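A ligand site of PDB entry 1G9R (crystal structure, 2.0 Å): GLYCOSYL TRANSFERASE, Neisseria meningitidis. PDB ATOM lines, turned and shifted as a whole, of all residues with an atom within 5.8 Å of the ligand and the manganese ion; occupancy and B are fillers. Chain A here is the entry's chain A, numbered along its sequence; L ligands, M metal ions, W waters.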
ATOM      1  N   PHE A   5      -7.237 -31.910 -22.655  1.00  0.00           N
ATOM      2  CA  PHE A   5      -8.407 -31.126 -22.262  1.00  0.00           C
ATOM      3  C   PHE A   5      -9.175 -32.060 -21.333  1.00  0.00           C
ATOM      4  O   PHE A   5      -8.942 -33.279 -21.335  1.00  0.00           O
ATOM      5  CB  PHE A   5      -9.310 -30.838 -23.481  1.00  0.00           C
ATOM      6  CG  PHE A   5      -8.861 -29.701 -24.350  1.00  0.00           C
ATOM      7  CD1 PHE A   5      -8.892 -28.385 -23.875  1.00  0.00           C
ATOM      8  CD2 PHE A   5      -8.497 -29.923 -25.673  1.00  0.00           C
ATOM      9  CE1 PHE A   5      -8.567 -27.312 -24.723  1.00  0.00           C
ATOM     10  CE2 PHE A   5      -8.172 -28.850 -26.521  1.00  0.00           C
ATOM     11  CZ  PHE A   5      -8.217 -27.543 -26.041  1.00  0.00           C
ATOM     12  N   ALA A   6     -10.067 -31.498 -20.513  1.00  0.00           N
ATOM     13  CA  ALA A   6     -10.893 -32.291 -19.608  1.00  0.00           C
ATOM     14  C   ALA A   6     -12.282 -31.695 -19.747  1.00  0.00           C
ATOM     15  O   ALA A   6     -12.452 -30.467 -19.676  1.00  0.00           O
ATOM     16  CB  ALA A   6     -10.430 -32.153 -18.155  1.00  0.00           C
ATOM     17  N   ALA A   7     -13.282 -32.544 -19.932  1.00  0.00           N
ATOM     18  CA  ALA A   7     -14.632 -32.012 -20.074  1.00  0.00           C
ATOM     19  C   ALA A   7     -15.707 -33.035 -19.773  1.00  0.00           C
ATOM     20  O   ALA A   7     -15.498 -34.228 -19.966  1.00  0.00           O
ATOM     21  CB  ALA A   7     -14.836 -31.453 -21.485  1.00  0.00           C
ATOM     22  N   ASP A   8     -16.837 -32.543 -19.270  1.00  0.00           N
ATOM     23  CA  ASP A   8     -17.999 -33.379 -19.015  1.00  0.00           C
ATOM     24  C   ASP A   8     -18.936 -33.067 -20.191  1.00  0.00           C
ATOM     25  O   ASP A   8     -18.613 -32.231 -21.028  1.00  0.00           O
ATOM     26  CB  ASP A   8     -18.684 -33.051 -17.677  1.00  0.00           C
ATOM     27  CG  ASP A   8     -18.758 -31.566 -17.402  1.00  0.00           C
ATOM     28  OD1 ASP A   8     -18.823 -30.757 -18.360  1.00  0.00           O
ATOM     29  OD2 ASP A   8     -18.759 -31.212 -16.203  1.00  0.00           O
ATOM     30  N   ASN A  10     -21.560 -31.317 -20.446  1.00  0.00           N
ATOM     31  CA  ASN A  10     -21.944 -29.909 -20.487  1.00  0.00           C
ATOM     32  C   ASN A  10     -20.980 -29.037 -21.292  1.00  0.00           C
ATOM     33  O   ASN A  10     -21.408 -28.056 -21.916  1.00  0.00           O
ATOM     34  CB  ASN A  10     -22.045 -29.360 -19.064  1.00  0.00           C
ATOM     35  CG  ASN A  10     -22.469 -27.905 -19.021  1.00  0.00           C
ATOM     36  OD1 ASN A  10     -23.441 -27.516 -19.672  1.00  0.00           O
ATOM     37  ND2 ASN A  10     -21.748 -27.095 -18.260  1.00  0.00           N
ATOM     38  N   TYR A  11     -19.701 -29.375 -21.277  1.00  0.00           N
ATOM     39  CA  TYR A  11     -18.698 -28.580 -21.991  1.00  0.00           C
ATOM     40  C   TYR A  11     -18.239 -29.153 -23.325  1.00  0.00           C
ATOM     41  O   TYR A  11     -17.280 -28.653 -23.913  1.00  0.00           O
ATOM     42  CB  TYR A  11     -17.469 -28.370 -21.103  1.00  0.00           C
ATOM     43  CG  TYR A  11     -17.465 -27.079 -20.327  1.00  0.00           C
ATOM     44  CD1 TYR A  11     -18.659 -26.441 -19.968  1.00  0.00           C
ATOM     45  CD2 TYR A  11     -16.263 -26.487 -19.938  1.00  0.00           C
ATOM     46  CE1 TYR A  11     -18.650 -25.249 -19.246  1.00  0.00           C
ATOM     47  CE2 TYR A  11     -16.246 -25.304 -19.208  1.00  0.00           C
ATOM     48  CZ  TYR A  11     -17.445 -24.692 -18.869  1.00  0.00           C
ATOM     49  OH  TYR A  11     -17.411 -23.517 -18.162  1.00  0.00           O
ATOM     50  N   ILE A  76     -16.769 -22.934  -6.244  1.00  0.00           N
ATOM     51  CA  ILE A  76     -16.917 -22.035  -7.392  1.00  0.00           C
ATOM     52  C   ILE A  76     -18.022 -22.584  -8.286  1.00  0.00           C
ATOM     53  O   ILE A  76     -17.859 -23.599  -8.966  1.00  0.00           O
ATOM     54  CB  ILE A  76     -15.596 -21.909  -8.185  1.00  0.00           C
ATOM     55  CG1 ILE A  76     -14.462 -21.488  -7.229  1.00  0.00           C
ATOM     56  CG2 ILE A  76     -15.735 -20.864  -9.297  1.00  0.00           C
ATOM     57  CD1 ILE A  76     -13.101 -21.285  -7.902  1.00  0.00           C
ATOM     58  N   HIS A  78     -19.490 -21.940 -11.267  1.00  0.00           N
ATOM     59  CA  HIS A  78     -19.381 -22.270 -12.690  1.00  0.00           C
ATOM     60  C   HIS A  78     -18.446 -23.429 -12.994  1.00  0.00           C
ATOM     61  O   HIS A  78     -18.280 -23.813 -14.141  1.00  0.00           O
ATOM     62  CB  HIS A  78     -18.940 -21.046 -13.515  1.00  0.00           C
ATOM     63  CG  HIS A  78     -17.512 -20.654 -13.320  1.00  0.00           C
ATOM     64  ND1 HIS A  78     -17.085 -19.833 -12.304  1.00  0.00           N
ATOM     65  CD2 HIS A  78     -16.389 -20.986 -14.020  1.00  0.00           C
ATOM     66  CE1 HIS A  78     -15.777 -19.675 -12.375  1.00  0.00           C
ATOM     67  NE2 HIS A  78     -15.327 -20.366 -13.410  1.00  0.00           N
ATOM     68  N   ILE A  79     -17.855 -24.016 -11.956  1.00  0.00           N
ATOM     69  CA  ILE A  79     -16.945 -25.134 -12.162  1.00  0.00           C
ATOM     70  C   ILE A  79     -17.474 -26.472 -11.684  1.00  0.00           C
ATOM     71  O   ILE A  79     -17.873 -26.616 -10.536  1.00  0.00           O
ATOM     72  CB  ILE A  79     -15.599 -24.869 -11.463  1.00  0.00           C
ATOM     73  CG1 ILE A  79     -14.998 -23.563 -11.968  1.00  0.00           C
ATOM     74  CG2 ILE A  79     -14.635 -26.016 -11.723  1.00  0.00           C
ATOM     75  CD1 ILE A  79     -13.810 -23.079 -11.147  1.00  0.00           C
ATOM     76  N   SER A  80     -17.475 -27.465 -12.579  1.00  0.00           N
ATOM     77  CA  SER A  80     -17.940 -28.802 -12.233  1.00  0.00           C
ATOM     78  C   SER A  80     -16.771 -29.620 -11.671  1.00  0.00           C
ATOM     79  O   SER A  80     -15.608 -29.198 -11.741  1.00  0.00           O
ATOM     80  CB  SER A  80     -18.507 -29.495 -13.456  1.00  0.00           C
ATOM     81  OG  SER A  80     -17.476 -29.787 -14.375  1.00  0.00           O
ATOM     82  N   THR A  82     -15.325 -32.103 -12.749  1.00  0.00           N
ATOM     83  CA  THR A  82     -14.379 -32.531 -13.777  1.00  0.00           C
ATOM     84  C   THR A  82     -13.037 -31.774 -13.697  1.00  0.00           C
ATOM     85  O   THR A  82     -12.000 -32.271 -14.151  1.00  0.00           O
ATOM     86  CB  THR A  82     -14.991 -32.339 -15.188  1.00  0.00           C
ATOM     87  OG1 THR A  82     -16.134 -33.190 -15.323  1.00  0.00           O
ATOM     88  CG2 THR A  82     -13.985 -32.682 -16.276  1.00  0.00           C
ATOM     89  N   THR A  83     -13.075 -30.585 -13.122  1.00  0.00           N
ATOM     90  CA  THR A  83     -11.899 -29.738 -12.962  1.00  0.00           C
ATOM     91  C   THR A  83     -10.746 -30.444 -12.206  1.00  0.00           C
ATOM     92  O   THR A  83      -9.574 -30.070 -12.331  1.00  0.00           O
ATOM     93  CB  THR A  83     -12.288 -28.418 -12.225  1.00  0.00           C
ATOM     94  OG1 THR A  83     -11.232 -27.447 -12.357  1.00  0.00           O
ATOM     95  CG2 THR A  83     -12.555 -28.666 -10.757  1.00  0.00           C
ATOM     96  N   ARG A  86      -7.572 -33.565 -13.843  1.00  0.00           N
ATOM     97  CA  ARG A  86      -6.186 -33.314 -14.220  1.00  0.00           C
ATOM     98  C   ARG A  86      -5.194 -33.885 -13.202  1.00  0.00           C
ATOM     99  O   ARG A  86      -4.051 -34.182 -13.542  1.00  0.00           O
ATOM    100  CB  ARG A  86      -5.971 -31.811 -14.418  1.00  0.00           C
ATOM    101  CG  ARG A  86      -6.116 -30.970 -13.171  1.00  0.00           C
ATOM    102  CD  ARG A  86      -6.117 -29.480 -13.534  1.00  0.00           C
ATOM    103  NE  ARG A  86      -7.469 -28.974 -13.758  1.00  0.00           N
ATOM    104  CZ  ARG A  86      -7.753 -27.730 -14.159  1.00  0.00           C
ATOM    105  NH1 ARG A  86      -6.765 -26.872 -14.394  1.00  0.00           N
ATOM    106  NH2 ARG A  86      -9.020 -27.334 -14.261  1.00  0.00           N
ATOM    107  N   TYR A 101      -1.531 -29.229 -21.034  1.00  0.00           N
ATOM    108  CA  TYR A 101      -2.903 -29.193 -20.573  1.00  0.00           C
ATOM    109  C   TYR A 101      -3.501 -27.804 -20.725  1.00  0.00           C
ATOM    110  O   TYR A 101      -2.874 -26.795 -20.351  1.00  0.00           O
ATOM    111  CB  TYR A 101      -2.979 -29.619 -19.088  1.00  0.00           C
ATOM    112  CG  TYR A 101      -4.338 -29.315 -18.500  1.00  0.00           C
ATOM    113  CD1 TYR A 101      -5.379 -30.246 -18.548  1.00  0.00           C
ATOM    114  CD2 TYR A 101      -4.626 -28.046 -17.992  1.00  0.00           C
ATOM    115  CE1 TYR A 101      -6.671 -29.920 -18.122  1.00  0.00           C
ATOM    116  CE2 TYR A 101      -5.911 -27.703 -17.579  1.00  0.00           C
ATOM    117  CZ  TYR A 101      -6.921 -28.643 -17.653  1.00  0.00           C
ATOM    118  OH  TYR A 101      -8.202 -28.258 -17.276  1.00  0.00           O
ATOM    119  N   LEU A 102      -4.720 -27.746 -21.245  1.00  0.00           N
ATOM    120  CA  LEU A 102      -5.442 -26.489 -21.431  1.00  0.00           C
ATOM    121  C   LEU A 102      -6.850 -26.607 -20.857  1.00  0.00           C
ATOM    122  O   LEU A 102      -7.470 -27.667 -20.954  1.00  0.00           O
ATOM    123  CB  LEU A 102      -5.553 -26.145 -22.923  1.00  0.00           C
ATOM    124  CG  LEU A 102      -4.256 -25.936 -23.683  1.00  0.00           C
ATOM    125  CD1 LEU A 102      -4.564 -25.703 -25.143  1.00  0.00           C
ATOM    126  CD2 LEU A 102      -3.485 -24.756 -23.080  1.00  0.00           C
ATOM    127  N   ASP A 103      -7.345 -25.526 -20.261  1.00  0.00           N
ATOM    128  CA  ASP A 103      -8.704 -25.460 -19.736  1.00  0.00           C
ATOM    129  C   ASP A 103      -9.579 -25.383 -20.995  1.00  0.00           C
ATOM    130  O   ASP A 103      -9.076 -25.131 -22.090  1.00  0.00           O
ATOM    131  CB  ASP A 103      -8.910 -24.192 -18.914  1.00  0.00           C
ATOM    132  CG  ASP A 103      -8.766 -24.409 -17.413  1.00  0.00           C
ATOM    133  OD1 ASP A 103      -9.051 -23.462 -16.659  1.00  0.00           O
ATOM    134  OD2 ASP A 103      -8.364 -25.507 -16.973  1.00  0.00           O
ATOM    135  N   ILE A 104     -10.881 -25.547 -20.841  1.00  0.00           N
ATOM    136  CA  ILE A 104     -11.790 -25.507 -21.985  1.00  0.00           C
ATOM    137  C   ILE A 104     -12.081 -24.077 -22.425  1.00  0.00           C
ATOM    138  O   ILE A 104     -12.333 -23.814 -23.611  1.00  0.00           O
ATOM    139  CB  ILE A 104     -13.118 -26.195 -21.631  1.00  0.00           C
ATOM    140  CG1 ILE A 104     -12.863 -27.671 -21.343  1.00  0.00           C
ATOM    141  CG2 ILE A 104     -14.147 -25.988 -22.749  1.00  0.00           C
ATOM    142  CD1 ILE A 104     -12.284 -28.466 -22.506  1.00  0.00           C
ATOM    143  N   ASP A 105     -12.046 -23.150 -21.471  1.00  0.00           N
ATOM    144  CA  ASP A 105     -12.325 -21.742 -21.742  1.00  0.00           C
ATOM    145  C   ASP A 105     -11.100 -20.979 -22.233  1.00  0.00           C
ATOM    146  O   ASP A 105     -10.797 -19.900 -21.721  1.00  0.00           O
ATOM    147  CB  ASP A 105     -12.875 -21.074 -20.478  1.00  0.00           C
ATOM    148  CG  ASP A 105     -11.906 -21.128 -19.311  1.00  0.00           C
ATOM    149  OD1 ASP A 105     -11.016 -22.017 -19.313  1.00  0.00           O
ATOM    150  OD2 ASP A 105     -12.027 -20.311 -18.385  1.00  0.00           O
ATOM    151  N   VAL A 106     -10.402 -21.535 -23.221  1.00  0.00           N
ATOM    152  CA  VAL A 106      -9.254 -20.857 -23.792  1.00  0.00           C
ATOM    153  C   VAL A 106      -9.446 -20.702 -25.295  1.00  0.00           C
ATOM    154  O   VAL A 106     -10.204 -21.441 -25.927  1.00  0.00           O
ATOM    155  CB  VAL A 106      -7.921 -21.632 -23.560  1.00  0.00           C
ATOM    156  CG1 VAL A 106      -7.729 -21.928 -22.075  1.00  0.00           C
ATOM    157  CG2 VAL A 106      -7.898 -22.902 -24.400  1.00  0.00           C
ATOM    158  N   ASP A 130      -0.570 -16.357 -11.826  1.00  0.00           N
ATOM    159  CA  ASP A 130      -1.915 -15.804 -11.690  1.00  0.00           C
ATOM    160  C   ASP A 130      -1.777 -14.482 -10.942  1.00  0.00           C
ATOM    161  O   ASP A 130      -1.613 -14.470  -9.716  1.00  0.00           O
ATOM    162  CB  ASP A 130      -2.825 -16.759 -10.909  1.00  0.00           C
ATOM    163  CG  ASP A 130      -4.276 -16.354 -10.993  1.00  0.00           C
ATOM    164  OD1 ASP A 130      -4.590 -15.169 -10.732  1.00  0.00           O
ATOM    165  OD2 ASP A 130      -5.101 -17.229 -11.324  1.00  0.00           O
ATOM    166  N   ASN A 153      -1.509 -20.100 -12.381  1.00  0.00           N
ATOM    167  CA  ASN A 153      -2.873 -20.411 -12.785  1.00  0.00           C
ATOM    168  C   ASN A 153      -2.829 -21.812 -13.402  1.00  0.00           C
ATOM    169  O   ASN A 153      -1.932 -22.128 -14.169  1.00  0.00           O
ATOM    170  CB  ASN A 153      -3.383 -19.368 -13.795  1.00  0.00           C
ATOM    171  CG  ASN A 153      -4.812 -19.632 -14.224  1.00  0.00           C
ATOM    172  OD1 ASN A 153      -5.050 -20.304 -15.216  1.00  0.00           O
ATOM    173  ND2 ASN A 153      -5.759 -19.125 -13.452  1.00  0.00           N
ATOM    174  N   ALA A 154      -3.808 -22.642 -13.042  1.00  0.00           N
ATOM    175  CA  ALA A 154      -3.850 -24.015 -13.539  1.00  0.00           C
ATOM    176  C   ALA A 154      -4.491 -24.217 -14.909  1.00  0.00           C
ATOM    177  O   ALA A 154      -4.613 -25.352 -15.387  1.00  0.00           O
ATOM    178  CB  ALA A 154      -4.561 -24.888 -12.512  1.00  0.00           C
ATOM    179  N   GLY A 155      -4.900 -23.128 -15.555  1.00  0.00           N
ATOM    180  CA  GLY A 155      -5.544 -23.237 -16.855  1.00  0.00           C
ATOM    181  C   GLY A 155      -4.671 -23.588 -18.049  1.00  0.00           C
ATOM    182  O   GLY A 155      -5.187 -23.989 -19.099  1.00  0.00           O
ATOM    183  N   TYR A 186      -9.331 -22.013  -4.194  1.00  0.00           N
ATOM    184  CA  TYR A 186      -9.289 -22.280  -5.623  1.00  0.00           C
ATOM    185  C   TYR A 186      -9.220 -23.733  -6.064  1.00  0.00           C
ATOM    186  O   TYR A 186      -8.650 -24.052  -7.105  1.00  0.00           O
ATOM    187  CB  TYR A 186      -8.177 -21.443  -6.258  1.00  0.00           C
ATOM    188  CG  TYR A 186      -8.355 -19.962  -6.007  1.00  0.00           C
ATOM    189  CD1 TYR A 186      -7.609 -19.314  -5.022  1.00  0.00           C
ATOM    190  CD2 TYR A 186      -9.298 -19.217  -6.725  1.00  0.00           C
ATOM    191  CE1 TYR A 186      -7.801 -17.953  -4.755  1.00  0.00           C
ATOM    192  CE2 TYR A 186      -9.498 -17.858  -6.463  1.00  0.00           C
ATOM    193  CZ  TYR A 186      -8.739 -17.240  -5.473  1.00  0.00           C
ATOM    194  OH  TYR A 186      -8.926 -15.901  -5.207  1.00  0.00           O
ATOM    195  N   GLN A 187      -9.790 -24.616  -5.263  1.00  0.00           N
ATOM    196  CA  GLN A 187      -9.900 -26.030  -5.592  1.00  0.00           C
ATOM    197  C   GLN A 187      -8.636 -26.711  -6.154  1.00  0.00           C
ATOM    198  O   GLN A 187      -7.579 -26.690  -5.522  1.00  0.00           O
ATOM    199  CB  GLN A 187     -11.099 -26.167  -6.545  1.00  0.00           C
ATOM    200  CG  GLN A 187     -12.323 -25.415  -5.989  1.00  0.00           C
ATOM    201  CD  GLN A 187     -13.518 -25.311  -6.940  1.00  0.00           C
ATOM    202  OE1 GLN A 187     -14.624 -24.999  -6.515  1.00  0.00           O
ATOM    203  NE2 GLN A 187     -13.293 -25.542  -8.235  1.00  0.00           N
ATOM    204  N   ASP A 188      -8.737 -27.318  -7.334  1.00  0.00           N
ATOM    205  CA  ASP A 188      -7.600 -28.023  -7.918  1.00  0.00           C
ATOM    206  C   ASP A 188      -6.355 -27.162  -8.120  1.00  0.00           C
ATOM    207  O   ASP A 188      -5.216 -27.640  -8.059  1.00  0.00           O
ATOM    208  CB  ASP A 188      -7.980 -28.660  -9.253  1.00  0.00           C
ATOM    209  CG  ASP A 188      -8.454 -27.637 -10.256  1.00  0.00           C
ATOM    210  OD1 ASP A 188      -9.604 -27.161 -10.119  1.00  0.00           O
ATOM    211  OD2 ASP A 188      -7.677 -27.294 -11.168  1.00  0.00           O
ATOM    212  N   GLN A 189      -6.584 -25.876  -8.379  1.00  0.00           N
ATOM    213  CA  GLN A 189      -5.493 -24.931  -8.592  1.00  0.00           C
ATOM    214  C   GLN A 189      -4.645 -24.807  -7.328  1.00  0.00           C
ATOM    215  O   GLN A 189      -3.421 -24.721  -7.399  1.00  0.00           O
ATOM    216  CB  GLN A 189      -6.086 -23.577  -8.997  1.00  0.00           C
ATOM    217  CG  GLN A 189      -5.072 -22.515  -9.380  1.00  0.00           C
ATOM    218  CD  GLN A 189      -5.760 -21.323 -10.018  1.00  0.00           C
ATOM    219  OE1 GLN A 189      -5.822 -21.214 -11.247  1.00  0.00           O
ATOM    220  NE2 GLN A 189      -6.316 -20.441  -9.186  1.00  0.00           N
ATOM    221  N   MET A 210      -5.270 -13.608 -19.001  1.00  0.00           N
ATOM    222  CA  MET A 210      -6.603 -13.543 -18.406  1.00  0.00           C
ATOM    223  C   MET A 210      -7.093 -12.116 -18.184  1.00  0.00           C
ATOM    224  O   MET A 210      -6.362 -11.156 -18.408  1.00  0.00           O
ATOM    225  CB  MET A 210      -6.571 -14.308 -17.065  1.00  0.00           C
ATOM    226  CG  MET A 210      -6.233 -15.787 -17.227  1.00  0.00           C
ATOM    227  SD  MET A 210      -5.674 -16.675 -15.567  1.00  0.00           S
ATOM    228  CE  MET A 210      -3.815 -16.172 -15.592  1.00  0.00           C
ATOM    229  N   HIS A 244      -7.370 -16.677 -22.003  1.00  0.00           N
ATOM    230  CA  HIS A 244      -7.989 -17.557 -21.022  1.00  0.00           C
ATOM    231  C   HIS A 244      -9.069 -16.771 -20.271  1.00  0.00           C
ATOM    232  O   HIS A 244      -8.764 -15.864 -19.498  1.00  0.00           O
ATOM    233  CB  HIS A 244      -6.943 -18.088 -20.042  1.00  0.00           C
ATOM    234  CG  HIS A 244      -7.492 -19.016 -19.007  1.00  0.00           C
ATOM    235  ND1 HIS A 244      -6.749 -19.433 -17.914  1.00  0.00           N
ATOM    236  CD2 HIS A 244      -8.703 -19.611 -18.891  1.00  0.00           C
ATOM    237  CE1 HIS A 244      -7.494 -20.233 -17.164  1.00  0.00           C
ATOM    238  NE2 HIS A 244      -8.679 -20.360 -17.741  1.00  0.00           N
ATOM    239  N   TYR A 245     -10.320 -17.151 -20.481  1.00  0.00           N
ATOM    240  CA  TYR A 245     -11.452 -16.476 -19.860  1.00  0.00           C
ATOM    241  C   TYR A 245     -11.782 -17.000 -18.477  1.00  0.00           C
ATOM    242  O   TYR A 245     -12.927 -17.378 -18.191  1.00  0.00           O
ATOM    243  CB  TYR A 245     -12.648 -16.589 -20.806  1.00  0.00           C
ATOM    244  CG  TYR A 245     -12.322 -15.966 -22.135  1.00  0.00           C
ATOM    245  CD1 TYR A 245     -12.332 -14.571 -22.295  1.00  0.00           C
ATOM    246  CD2 TYR A 245     -11.892 -16.740 -23.208  1.00  0.00           C
ATOM    247  CE1 TYR A 245     -11.913 -13.980 -23.482  1.00  0.00           C
ATOM    248  CE2 TYR A 245     -11.467 -16.151 -24.403  1.00  0.00           C
ATOM    249  CZ  TYR A 245     -11.472 -14.768 -24.531  1.00  0.00           C
ATOM    250  OH  TYR A 245     -11.012 -14.169 -25.691  1.00  0.00           O
ATOM    251  N   CYS A 246     -10.755 -16.997 -17.631  1.00  0.00           N
ATOM    252  CA  CYS A 246     -10.852 -17.463 -16.250  1.00  0.00           C
ATOM    253  C   CYS A 246     -11.942 -16.665 -15.561  1.00  0.00           C
ATOM    254  O   CYS A 246     -12.049 -15.453 -15.745  1.00  0.00           O
ATOM    255  CB  CYS A 246      -9.496 -17.232 -15.557  1.00  0.00           C
ATOM    256  SG  CYS A 246      -9.342 -17.995 -13.925  1.00  0.00           S
ATOM    257  N   GLY A 247     -12.762 -17.331 -14.755  1.00  0.00           N
ATOM    258  CA  GLY A 247     -13.823 -16.627 -14.065  1.00  0.00           C
ATOM    259  C   GLY A 247     -15.201 -16.891 -14.661  1.00  0.00           C
ATOM    260  O   GLY A 247     -15.316 -17.538 -15.699  1.00  0.00           O
ATOM    261  N   PRO A 248     -16.264 -16.381 -14.026  1.00  0.00           N
ATOM    262  CA  PRO A 248     -17.635 -16.564 -14.490  1.00  0.00           C
ATOM    263  C   PRO A 248     -17.965 -16.064 -15.897  1.00  0.00           C
ATOM    264  O   PRO A 248     -18.825 -16.625 -16.571  1.00  0.00           O
ATOM    265  CB  PRO A 248     -18.450 -15.841 -13.411  1.00  0.00           C
ATOM    266  CG  PRO A 248     -17.532 -14.702 -13.033  1.00  0.00           C
ATOM    267  CD  PRO A 248     -16.206 -15.418 -12.915  1.00  0.00           C
ATOM    268  N   LYS A 250     -17.747 -16.084 -19.459  1.00  0.00           N
ATOM    269  CA  LYS A 250     -17.259 -16.927 -20.546  1.00  0.00           C
ATOM    270  C   LYS A 250     -17.588 -16.378 -21.930  1.00  0.00           C
ATOM    271  O   LYS A 250     -18.625 -15.746 -22.132  1.00  0.00           O
ATOM    272  CB  LYS A 250     -17.851 -18.335 -20.409  1.00  0.00           C
ATOM    273  CG  LYS A 250     -17.515 -19.038 -19.085  1.00  0.00           C
ATOM    274  CD  LYS A 250     -16.019 -19.139 -18.822  1.00  0.00           C
ATOM    275  CE  LYS A 250     -15.744 -19.924 -17.529  1.00  0.00           C
ATOM    276  NZ  LYS A 250     -14.328 -19.750 -17.056  1.00  0.00           N
HETATM  277  N1  LIG L   1     -15.481 -28.026 -16.581  1.00  0.00           N
HETATM  278  C1  LIG L   1     -16.256 -28.924 -17.327  1.00  0.00           C
HETATM  279  N2  LIG L   1     -17.624 -28.606 -17.311  1.00  0.00           N
HETATM  280  C2  LIG L   1     -18.248 -27.489 -16.641  1.00  0.00           C
HETATM  281  C3  LIG L   1     -17.376 -26.626 -15.903  1.00  0.00           C
HETATM  282  C4  LIG L   1     -16.077 -26.891 -15.884  1.00  0.00           C
HETATM  283  O1  LIG L   1     -15.772 -29.889 -17.918  1.00  0.00           O
HETATM  284  O2  LIG L   1     -19.451 -27.348 -16.717  1.00  0.00           O
HETATM  285  C5  LIG L   1     -13.955 -28.052 -16.346  1.00  0.00           C
HETATM  286  C6  LIG L   1     -13.283 -27.612 -17.634  1.00  0.00           C
HETATM  287  O3  LIG L   1     -12.275 -28.556 -18.016  1.00  0.00           O
HETATM  288  C7  LIG L   1     -12.722 -26.237 -17.297  1.00  0.00           C
HETATM  289  C8  LIG L   1     -12.228 -26.476 -15.879  1.00  0.00           C
HETATM  290  O4  LIG L   1     -13.284 -27.377 -15.310  1.00  0.00           O
HETATM  291  O5  LIG L   1     -11.696 -25.691 -18.106  1.00  0.00           O
HETATM  292  C9  LIG L   1     -12.492 -25.657 -14.648  1.00  0.00           C
HETATM  293  O6  LIG L   1     -13.030 -24.283 -14.777  1.00  0.00           O
HETATM  294  P1  LIG L   1     -12.959 -22.998 -15.737  1.00  0.00           P
HETATM  295  O7  LIG L   1     -12.133 -23.156 -16.951  1.00  0.00           O
HETATM  296  O8  LIG L   1     -14.346 -22.493 -16.037  1.00  0.00           O
HETATM  297  O9  LIG L   1     -12.219 -22.436 -14.449  1.00  0.00           O
HETATM  298  P2  LIG L   1     -11.525 -21.057 -14.056  1.00  0.00           P
HETATM  299  O10 LIG L   1     -10.676 -20.787 -15.236  1.00  0.00           O
HETATM  300  O11 LIG L   1     -12.584 -20.066 -13.903  1.00  0.00           O
HETATM  301  O12 LIG L   1     -10.638 -21.221 -12.773  1.00  0.00           O
HETATM  302  C10 LIG L   1      -9.149 -21.236 -12.159  1.00  0.00           C
HETATM  303  C11 LIG L   1      -8.344 -22.139 -13.176  1.00  0.00           C
HETATM  304  C12 LIG L   1      -9.012 -23.543 -13.618  1.00  0.00           C
HETATM  305  C13 LIG L   1      -9.392 -24.334 -12.326  1.00  0.00           C
HETATM  306  C14 LIG L   1     -10.220 -23.317 -11.415  1.00  0.00           C
HETATM  307  C15 LIG L   1     -10.427 -23.966 -10.056  1.00  0.00           C
HETATM  308  F1  LIG L   1      -7.999 -21.424 -14.341  1.00  0.00           F
HETATM  309  O13 LIG L   1      -8.071 -24.299 -14.314  1.00  0.00           O
HETATM  310  O14 LIG L   1      -8.177 -24.777 -11.660  1.00  0.00           O
HETATM  311  O15 LIG L   1      -9.484 -22.043 -11.021  1.00  0.00           O
HETATM  312  O16 LIG L   1     -11.077 -25.188  -9.829  1.00  0.00           O
HETATM  313 MN    MN M   1     -10.350 -21.808 -17.161  1.00  0.00          MN
HETATM  314  O   HOH W   1      -9.715 -28.797 -20.128  1.00  0.00           O
HETATM  315  O   HOH W   2     -12.762 -19.059 -11.011  1.00  0.00           O
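The side-chain carboxylate (OD1) of Asp 8 sits at hydrogen-bond distance from a nitrogen (N2) of the ligand (2.7 Å).
An oxygen (O5) of the ligand is in hydrogen-bond range of the backbone NH (N) of Ile 104 (2.9 Å).
The backbone carbonyl oxygen of Ala 6 lies within hydrogen-bond range of an oxygen (O3) of the ligand (2.5 Å).
The side-chain hydroxyl (OG) of Ser 80 is in hydrogen-bond range of a nitrogen (N2) of the ligand (3.2 Å).
The side-chain sulfur (SG) of Cys 246 lies within hydrogen-bond range of an oxygen (O12) of the ligand, at 3.7 Å.
The guanidinium group (NH1) of Arg 86 lies within hydrogen-bond range of an oxygen (O13) of the ligand (2.9 Å).
The backbone NH of Asp 8 lies within hydrogen-bond range of an oxygen (O1) of the ligand (3.2 Å).
The side-chain hydroxyl (OG1) of Thr 83 sits close to an oxygen (O16) of the ligand (3.4 Å).
NE2 of His 78 is in hydrogen-bond range of O11 of the ligand, at 2.8 Å.
The side-chain amino group of Lys 250 lies within salt-bridge range of an oxygen (O8) of the ligand.
An oxygen (O2) of the ligand lies within hydrogen-bond range of the side-chain amide nitrogen (ND2) of Asn 10 (2.8 Å).
An oxygen (O11) of the ligand is in hydrogen-bond range of the backbone NH of Gly 247.
OD1 of Asp 188 is in hydrogen-bond range of O16 of the ligand (2.5 Å).
NE2 of Gln 187 sits at hydrogen-bond distance from O16 of the ligand (2.8 Å).
The manganese ion is bound by OD1 of Asp 103, O10 of the ligand, O7 of the ligand, OD1 of Asp 105, NE2 of His 244 and OD2 of Asp 105.
The manganese ion has six donor atoms within binding distance.
Of the 34 residues printed, 3 come within 4 Å of the manganese ion.
Along chain A the residues within 4 Å of the manganese ion span positions 103 to 244.
The nearest printed residue that does not touch the manganese ion is Cys 246 (4.5 Å).
The side-chain amino group (NZ) of Lys 250 sits at hydrogen-bond distance from the backbone carbonyl oxygen (O) of Tyr 245 (3.0 Å).
The side-chain amide oxygen (OD1) of Asn 153 is in hydrogen-bond range of the backbone NH (N) of Gly 155, at 2.8 Å.
The backbone NH (N) of Tyr 11 is in hydrogen-bond range of the side-chain carboxylate (OD1) of Asp 8, at 3.3 Å.
The backbone carbonyl oxygen (O) of Ala 154 lies within hydrogen-bond range of the guanidinium group (NH1) of Arg 86.
The backbone NH (N) of Ala 154 sits at hydrogen-bond distance from the side-chain amide oxygen (OE1) of Gln 189.
The backbone NH (N) of Tyr 245 sits at hydrogen-bond distance from the backbone carbonyl oxygen (O) of Asp 105, at 3.1 Å.
The side-chain hydroxyl (OH) of Tyr 101 is in hydrogen-bond range of the side-chain carboxylate (OD2) of Asp 103.
The side-chain carboxylate (OD2) of Asp 8 lies within hydrogen-bond range of the side-chain hydroxyl (OG1) of Thr 82, at 3.4 Å.
OD1 of Asn 153 lies close to F1 of the ligand.
Merely in contact with the ligand: Ala 7, Gln 189, Tyr 11, Tyr 186, Ile 79, Gly 155, Ala 154 and Thr 82.
25 residues have an atom within 4 Å of the ligand: Ala 6, Ala 7, Asp 8, Asn 10, Tyr 11, His 78, Ile 79, Ser 80, Thr 82, Thr 83, Arg 86, Asp 103, Ile 104, Asp 105, Asn 153, Ala 154, Gly 155, Tyr 186, Gln 187, Asp 188, Gln 189, His 244, Cys 246, Gly 247 and Lys 250.
Water W1 lies within hydrogen-bond range of the backbone carbonyl oxygen (O) of Leu 102 (2.6 Å), the backbone NH (N) of Ala 6 (2.8 Å), the side-chain hydroxyl (OH) of Tyr 101 (3.3 Å) and an oxygen (O3) of the ligand (3.3 Å).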
